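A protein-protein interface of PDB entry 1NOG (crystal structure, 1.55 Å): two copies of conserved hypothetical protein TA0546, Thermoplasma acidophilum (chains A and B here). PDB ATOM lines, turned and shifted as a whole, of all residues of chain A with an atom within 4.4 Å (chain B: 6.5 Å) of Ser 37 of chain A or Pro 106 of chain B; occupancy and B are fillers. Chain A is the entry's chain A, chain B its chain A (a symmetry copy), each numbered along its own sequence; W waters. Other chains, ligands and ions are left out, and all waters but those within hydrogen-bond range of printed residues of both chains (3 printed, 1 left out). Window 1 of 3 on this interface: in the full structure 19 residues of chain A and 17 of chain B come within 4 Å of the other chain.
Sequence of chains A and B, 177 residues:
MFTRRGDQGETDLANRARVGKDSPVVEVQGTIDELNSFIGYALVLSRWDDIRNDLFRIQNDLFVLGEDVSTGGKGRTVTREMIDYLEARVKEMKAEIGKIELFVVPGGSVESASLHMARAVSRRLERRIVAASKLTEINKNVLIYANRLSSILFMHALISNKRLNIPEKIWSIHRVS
No position is printed for both chains. Of the 12 pairs that touch across the chains among the printed residues, none has its exchanged pair printed and touching as well.
Of the printed residues of chain B, Asp 33 of chain A touches Ala 120 (3.4 Å). Printed residues of chain B within 4 Å of Glu 34 of chain A: Ala 120 (3.5 Å). Of the printed residues of chain A, Val 105 of chain B touches Gln 59. Printed residues of chain A within 4 Å of Ala 113 of chain B: Tyr 41. Printed residues of chain A within 4 Å of His 116 of chain B: Ser 37. The nearest printed residue of chain B that does not touch Ser 37 of chain A is Ala 120 of chain B (4.04 Å).
Water W3 bridges OE1 of Gln 59 of chain A and O of Pro 106 of chain B. Water W1 bridges the backbone carbonyl oxygen (O) of Gly 40 of chain A (2.9 Å) and the backbone NH (N) of Gly 108 of chain B (2.9 Å). Water W2 lies within hydrogen-bond range of the side-chain carboxylate of Asp 33 of chain A and the backbone carbonyl oxygen of His 116 of chain B.
Hydrophobic or aromatic side chains of chain A within 4 Å of the printed part of chain B: Phe 38 and Tyr 41. Printed residues of chain B that touch a printed residue of chain A: Val 105, Pro 106, Ala 113, His 116, Met 117 and Ala 120. Hydrophobic or aromatic side chains of chain B that line the printed part of chain A: Val 105, Pro 106, Ala 113, Met 117 and Ala 120.
The side-chain hydroxyl of Ser 37 of chain A is in hydrogen-bond range of the backbone carbonyl oxygen of Glu 34 of chain A. OD1 of Asn 36 of chain A sits at hydrogen-bond distance from NE2 of Gln 59 of chain A, 3.0 Å away. The backbone NH (N) of Gly 40 of chain A lies close to the side-chain amide nitrogen (NE2) of Gln 59 of chain A (3.4 Å). The backbone NH of Val 105 of chain B is in hydrogen-bond range of the backbone carbonyl oxygen of Lys 169 of chain B (2.8 Å). The backbone carbonyl oxygen (O) of Ser 112 of chain B lies within hydrogen-bond range of a ring nitrogen (ND1) of His 116 of chain B.
Asp 33 of chain A touches Ala 120 of chain B. Glu 34 of chain A touches Ala 120 of chain B. Pro 106 of chain B touches Asn 36 of chain A. Ser 37 of chain A touches Pro 106 of chain B (N to CG, 3.9 Å). CB of Ser 37 of chain A touches O of His 116 of chain B, at 3.7 Å. Met 117 of chain B touches Ser 37 of chain A (CG to OG, 3.4 Å). Met 117 of chain B touches Phe 38 of chain A. Gly 40 of chain A touches Pro 106 of chain B (CA to O, 3.3 Å). CA of Tyr 41 of chain A touches CB of Ala 113 of chain B, at 3.8 Å. CE of Met 117 of chain B touches CG of Tyr 41 of chain A, 3.5 Å away.
NE2 of Gln 59 of chain A sits at hydrogen-bond distance from O of Pro 106 of chain B, 2.9 Å away.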
ATOM      1  N   ASP A  33     -16.999 -21.847  19.716  1.00  0.00           N
ATOM      2  CA  ASP A  33     -18.216 -21.135  19.350  1.00  0.00           C
ATOM      3  C   ASP A  33     -19.271 -21.248  20.446  1.00  0.00           C
ATOM      4  O   ASP A  33     -19.898 -20.258  20.826  1.00  0.00           O
ATOM      5  CB  ASP A  33     -18.775 -21.698  18.044  1.00  0.00           C
ATOM      6  CG  ASP A  33     -20.182 -21.224  17.765  1.00  0.00           C
ATOM      7  OD1 ASP A  33     -20.377 -20.004  17.586  1.00  0.00           O
ATOM      8  OD2 ASP A  33     -21.094 -22.075  17.734  1.00  0.00           O
ATOM      9  N   GLU A  34     -19.470 -22.463  20.947  1.00  0.00           N
ATOM     10  CA  GLU A  34     -20.451 -22.696  21.998  1.00  0.00           C
ATOM     11  C   GLU A  34     -20.059 -21.908  23.236  1.00  0.00           C
ATOM     12  O   GLU A  34     -20.895 -21.252  23.853  1.00  0.00           O
ATOM     13  CB  GLU A  34     -20.546 -24.185  22.347  1.00  0.00           C
ATOM     14  CG  GLU A  34     -21.748 -24.515  23.220  1.00  0.00           C
ATOM     15  CD  GLU A  34     -21.872 -25.991  23.525  1.00  0.00           C
ATOM     16  OE1 GLU A  34     -21.415 -26.807  22.700  1.00  0.00           O
ATOM     17  OE2 GLU A  34     -22.444 -26.333  24.583  1.00  0.00           O
ATOM     18  N   LEU A  35     -18.782 -21.975  23.601  1.00  0.00           N
ATOM     19  CA  LEU A  35     -18.306 -21.251  24.769  1.00  0.00           C
ATOM     20  C   LEU A  35     -18.555 -19.754  24.611  1.00  0.00           C
ATOM     21  O   LEU A  35     -19.036 -19.094  25.533  1.00  0.00           O
ATOM     22  CB  LEU A  35     -16.811 -21.506  24.977  1.00  0.00           C
ATOM     23  CG  LEU A  35     -16.136 -20.713  26.099  1.00  0.00           C
ATOM     24  CD1 LEU A  35     -16.834 -20.959  27.429  1.00  0.00           C
ATOM     25  CD2 LEU A  35     -14.676 -21.123  26.178  1.00  0.00           C
ATOM     26  N   ASN A  36     -18.238 -19.216  23.439  1.00  0.00           N
ATOM     27  CA  ASN A  36     -18.438 -17.793  23.207  1.00  0.00           C
ATOM     28  C   ASN A  36     -19.906 -17.409  23.430  1.00  0.00           C
ATOM     29  O   ASN A  36     -20.199 -16.346  23.982  1.00  0.00           O
ATOM     30  CB  ASN A  36     -18.005 -17.415  21.785  1.00  0.00           C
ATOM     31  CG  ASN A  36     -17.354 -16.042  21.722  1.00  0.00           C
ATOM     32  OD1 ASN A  36     -17.614 -15.183  22.563  1.00  0.00           O
ATOM     33  ND2 ASN A  36     -16.511 -15.827  20.716  1.00  0.00           N
ATOM     34  N   SER A  37     -20.827 -18.276  23.009  1.00  0.00           N
ATOM     35  CA  SER A  37     -22.251 -17.994  23.176  1.00  0.00           C
ATOM     36  C   SER A  37     -22.648 -18.012  24.650  1.00  0.00           C
ATOM     37  O   SER A  37     -23.468 -17.205  25.088  1.00  0.00           O
ATOM     38  CB  SER A  37     -23.104 -19.000  22.390  1.00  0.00           C
ATOM     39  OG  SER A  37     -23.096 -20.289  22.985  1.00  0.00           O
ATOM     40  N   PHE A  38     -22.069 -18.933  25.416  1.00  0.00           N
ATOM     41  CA  PHE A  38     -22.374 -19.014  26.846  1.00  0.00           C
ATOM     42  C   PHE A  38     -21.797 -17.797  27.570  1.00  0.00           C
ATOM     43  O   PHE A  38     -22.398 -17.290  28.520  1.00  0.00           O
ATOM     44  CB  PHE A  38     -21.805 -20.298  27.468  1.00  0.00           C
ATOM     45  CG  PHE A  38     -22.711 -21.492  27.340  1.00  0.00           C
ATOM     46  CD1 PHE A  38     -22.952 -22.078  26.099  1.00  0.00           C
ATOM     47  CD2 PHE A  38     -23.328 -22.029  28.465  1.00  0.00           C
ATOM     48  CE1 PHE A  38     -23.796 -23.190  25.982  1.00  0.00           C
ATOM     49  CE2 PHE A  38     -24.173 -23.140  28.360  1.00  0.00           C
ATOM     50  CZ  PHE A  38     -24.406 -23.720  27.116  1.00  0.00           C
ATOM     51  N   ILE A  39     -20.628 -17.337  27.132  1.00  0.00           N
ATOM     52  CA  ILE A  39     -20.014 -16.163  27.744  1.00  0.00           C
ATOM     53  C   ILE A  39     -20.879 -14.938  27.450  1.00  0.00           C
ATOM     54  O   ILE A  39     -21.067 -14.078  28.313  1.00  0.00           O
ATOM     55  CB  ILE A  39     -18.583 -15.918  27.195  1.00  0.00           C
ATOM     56  CG1 ILE A  39     -17.658 -17.059  27.619  1.00  0.00           C
ATOM     57  CG2 ILE A  39     -18.045 -14.578  27.701  1.00  0.00           C
ATOM     58  CD1 ILE A  39     -17.577 -17.271  29.098  1.00  0.00           C
ATOM     59  N   GLY A  40     -21.407 -14.860  26.230  1.00  0.00           N
ATOM     60  CA  GLY A  40     -22.253 -13.733  25.869  1.00  0.00           C
ATOM     61  C   GLY A  40     -23.491 -13.679  26.741  1.00  0.00           C
ATOM     62  O   GLY A  40     -23.987 -12.604  27.072  1.00  0.00           O
ATOM     63  N   TYR A  41     -23.998 -14.850  27.104  1.00  0.00           N
ATOM     64  CA  TYR A  41     -25.170 -14.946  27.962  1.00  0.00           C
ATOM     65  C   TYR A  41     -24.801 -14.447  29.364  1.00  0.00           C
ATOM     66  O   TYR A  41     -25.509 -13.631  29.954  1.00  0.00           O
ATOM     67  CB  TYR A  41     -25.641 -16.404  28.019  1.00  0.00           C
ATOM     68  CG  TYR A  41     -26.898 -16.635  28.823  1.00  0.00           C
ATOM     69  CD1 TYR A  41     -28.093 -16.007  28.481  1.00  0.00           C
ATOM     70  CD2 TYR A  41     -26.897 -17.498  29.919  1.00  0.00           C
ATOM     71  CE1 TYR A  41     -29.265 -16.231  29.212  1.00  0.00           C
ATOM     72  CE2 TYR A  41     -28.059 -17.729  30.656  1.00  0.00           C
ATOM     73  CZ  TYR A  41     -29.237 -17.092  30.297  1.00  0.00           C
ATOM     74  OH  TYR A  41     -30.385 -17.308  31.030  1.00  0.00           O
ATOM     75  N   GLN A  59     -14.409 -12.810  24.837  1.00  0.00           N
ATOM     76  CA  GLN A  59     -15.137 -13.130  23.617  1.00  0.00           C
ATOM     77  C   GLN A  59     -14.294 -12.798  22.396  1.00  0.00           C
ATOM     78  O   GLN A  59     -14.290 -13.538  21.412  1.00  0.00           O
ATOM     79  CB  GLN A  59     -16.461 -12.372  23.568  1.00  0.00           C
ATOM     80  CG  GLN A  59     -17.458 -12.850  24.608  1.00  0.00           C
ATOM     81  CD  GLN A  59     -18.862 -12.398  24.282  1.00  0.00           C
ATOM     82  OE1 GLN A  59     -19.224 -11.243  24.496  1.00  0.00           O
ATOM     83  NE2 GLN A  59     -19.657 -13.307  23.734  1.00  0.00           N
ATOM     84  N   VAL B 104     -19.616 -11.728  14.158  1.00  0.00           N
ATOM     85  CA  VAL B 104     -20.507 -11.120  15.135  1.00  0.00           C
ATOM     86  C   VAL B 104     -20.191 -11.730  16.503  1.00  0.00           C
ATOM     87  O   VAL B 104     -20.099 -12.952  16.632  1.00  0.00           O
ATOM     88  CB  VAL B 104     -21.992 -11.410  14.797  1.00  0.00           C
ATOM     89  CG1 VAL B 104     -22.887 -10.962  15.945  1.00  0.00           C
ATOM     90  CG2 VAL B 104     -22.383 -10.690  13.516  1.00  0.00           C
ATOM     91  N   VAL B 105     -19.997 -10.884  17.509  1.00  0.00           N
ATOM     92  CA  VAL B 105     -19.726 -11.365  18.861  1.00  0.00           C
ATOM     93  C   VAL B 105     -21.102 -11.750  19.406  1.00  0.00           C
ATOM     94  O   VAL B 105     -21.987 -10.904  19.527  1.00  0.00           O
ATOM     95  CB  VAL B 105     -19.099 -10.258  19.736  1.00  0.00           C
ATOM     96  CG1 VAL B 105     -18.831 -10.792  21.138  1.00  0.00           C
ATOM     97  CG2 VAL B 105     -17.798  -9.764  19.101  1.00  0.00           C
ATOM     98  N   PRO B 106     -21.304 -13.034  19.742  1.00  0.00           N
ATOM     99  CA  PRO B 106     -22.609 -13.468  20.256  1.00  0.00           C
ATOM    100  C   PRO B 106     -23.035 -12.878  21.597  1.00  0.00           C
ATOM    101  O   PRO B 106     -22.340 -13.026  22.598  1.00  0.00           O
ATOM    102  CB  PRO B 106     -22.466 -14.987  20.300  1.00  0.00           C
ATOM    103  CG  PRO B 106     -21.015 -15.169  20.636  1.00  0.00           C
ATOM    104  CD  PRO B 106     -20.342 -14.153  19.733  1.00  0.00           C
ATOM    105  N   GLY B 107     -24.193 -12.221  21.609  1.00  0.00           N
ATOM    106  CA  GLY B 107     -24.695 -11.626  22.834  1.00  0.00           C
ATOM    107  C   GLY B 107     -25.581 -10.421  22.583  1.00  0.00           C
ATOM    108  O   GLY B 107     -26.300 -10.380  21.585  1.00  0.00           O
ATOM    109  N   GLY B 108     -25.541  -9.453  23.494  1.00  0.00           N
ATOM    110  CA  GLY B 108     -26.332  -8.240  23.338  1.00  0.00           C
ATOM    111  C   GLY B 108     -27.589  -8.178  24.181  1.00  0.00           C
ATOM    112  O   GLY B 108     -27.775  -7.261  24.984  1.00  0.00           O
ATOM    113  N   SER B 112     -31.191 -12.645  22.160  1.00  0.00           N
ATOM    114  CA  SER B 112     -30.184 -13.023  21.177  1.00  0.00           C
ATOM    115  C   SER B 112     -29.195 -14.037  21.739  1.00  0.00           C
ATOM    116  O   SER B 112     -28.808 -14.980  21.048  1.00  0.00           O
ATOM    117  CB  SER B 112     -29.442 -11.782  20.683  1.00  0.00           C
ATOM    118  OG  SER B 112     -30.326 -10.937  19.969  1.00  0.00           O
ATOM    119  N   ALA B 113     -28.794 -13.853  22.992  1.00  0.00           N
ATOM    120  CA  ALA B 113     -27.851 -14.775  23.616  1.00  0.00           C
ATOM    121  C   ALA B 113     -28.378 -16.208  23.617  1.00  0.00           C
ATOM    122  O   ALA B 113     -27.641 -17.145  23.306  1.00  0.00           O
ATOM    123  CB  ALA B 113     -27.545 -14.326  25.047  1.00  0.00           C
ATOM    124  N   SER B 114     -29.652 -16.380  23.958  1.00  0.00           N
ATOM    125  CA  SER B 114     -30.244 -17.717  23.993  1.00  0.00           C
ATOM    126  C   SER B 114     -30.297 -18.341  22.600  1.00  0.00           C
ATOM    127  O   SER B 114     -30.153 -19.554  22.445  1.00  0.00           O
ATOM    128  CB  SER B 114     -31.649 -17.667  24.608  1.00  0.00           C
ATOM    129  OG  SER B 114     -32.545 -16.894  23.824  1.00  0.00           O
ATOM    130  N   HIS B 116     -28.140 -17.687  20.180  1.00  0.00           N
ATOM    131  CA  HIS B 116     -26.776 -18.037  19.809  1.00  0.00           C
ATOM    132  C   HIS B 116     -26.371 -19.342  20.492  1.00  0.00           C
ATOM    133  O   HIS B 116     -25.634 -20.143  19.915  1.00  0.00           O
ATOM    134  CB  HIS B 116     -25.801 -16.919  20.183  1.00  0.00           C
ATOM    135  CG  HIS B 116     -25.689 -15.852  19.140  1.00  0.00           C
ATOM    136  ND1 HIS B 116     -26.046 -14.539  19.368  1.00  0.00           N
ATOM    137  CD2 HIS B 116     -25.270 -15.911  17.854  1.00  0.00           C
ATOM    138  CE1 HIS B 116     -25.849 -13.835  18.265  1.00  0.00           C
ATOM    139  NE2 HIS B 116     -25.379 -14.644  17.333  1.00  0.00           N
ATOM    140  N   MET B 117     -26.841 -19.563  21.721  1.00  0.00           N
ATOM    141  CA  MET B 117     -26.516 -20.811  22.410  1.00  0.00           C
ATOM    142  C   MET B 117     -27.202 -21.954  21.662  1.00  0.00           C
ATOM    143  O   MET B 117     -26.599 -22.998  21.428  1.00  0.00           O
ATOM    144  CB  MET B 117     -26.966 -20.773  23.876  1.00  0.00           C
ATOM    145  CG  MET B 117     -25.954 -20.086  24.805  1.00  0.00           C
ATOM    146  SD  MET B 117     -26.433 -20.029  26.578  1.00  0.00           S
ATOM    147  CE  MET B 117     -27.412 -19.100  26.409  1.00  0.00           C
ATOM    148  N   ALA B 118     -28.457 -21.746  21.269  1.00  0.00           N
ATOM    149  CA  ALA B 118     -29.191 -22.763  20.521  1.00  0.00           C
ATOM    150  C   ALA B 118     -28.467 -23.030  19.200  1.00  0.00           C
ATOM    151  O   ALA B 118     -28.346 -24.179  18.772  1.00  0.00           O
ATOM    152  CB  ALA B 118     -30.620 -22.291  20.250  1.00  0.00           C
ATOM    153  N   ALA B 120     -25.292 -22.777  18.560  1.00  0.00           N
ATOM    154  CA  ALA B 120     -24.082 -23.560  18.801  1.00  0.00           C
ATOM    155  C   ALA B 120     -24.424 -25.039  18.948  1.00  0.00           C
ATOM    156  O   ALA B 120     -23.688 -25.903  18.474  1.00  0.00           O
ATOM    157  CB  ALA B 120     -23.364 -23.054  20.047  1.00  0.00           C
ATOM    158  N   GLU B 168     -25.003  -4.764  17.001  1.00  0.00           N
ATOM    159  CA  GLU B 168     -24.143  -5.932  17.100  1.00  0.00           C
ATOM    160  C   GLU B 168     -22.717  -5.457  17.320  1.00  0.00           C
ATOM    161  O   GLU B 168     -22.343  -4.361  16.895  1.00  0.00           O
ATOM    162  CB  GLU B 168     -24.173  -6.754  15.809  1.00  0.00           C
ATOM    163  CG  GLU B 168     -25.489  -7.436  15.493  1.00  0.00           C
ATOM    164  CD  GLU B 168     -25.962  -8.354  16.603  1.00  0.00           C
ATOM    165  OE1 GLU B 168     -25.117  -8.939  17.312  1.00  0.00           O
ATOM    166  OE2 GLU B 168     -27.189  -8.498  16.755  1.00  0.00           O
ATOM    167  N   LYS B 169     -21.931  -6.277  18.003  1.00  0.00           N
ATOM    168  CA  LYS B 169     -20.527  -5.972  18.224  1.00  0.00           C
ATOM    169  C   LYS B 169     -19.797  -6.907  17.270  1.00  0.00           C
ATOM    170  O   LYS B 169     -20.179  -8.068  17.112  1.00  0.00           O
ATOM    171  CB  LYS B 169     -20.141  -6.234  19.680  1.00  0.00           C
ATOM    172  CG  LYS B 169     -20.803  -5.252  20.636  1.00  0.00           C
ATOM    173  CD  LYS B 169     -20.362  -5.450  22.072  1.00  0.00           C
ATOM    174  CE  LYS B 169     -20.904  -4.341  22.961  1.00  0.00           C
ATOM    175  NZ  LYS B 169     -20.486  -2.996  22.469  1.00  0.00           N
HETATM  176  O   HOH W   1     -23.685 -10.182  25.591  1.00  0.00           O
HETATM  177  O   HOH W   2     -23.204 -19.314  18.078  1.00  0.00           O
HETATM  178  O   HOH W   3     -21.577 -10.028  23.980  1.00  0.00           O
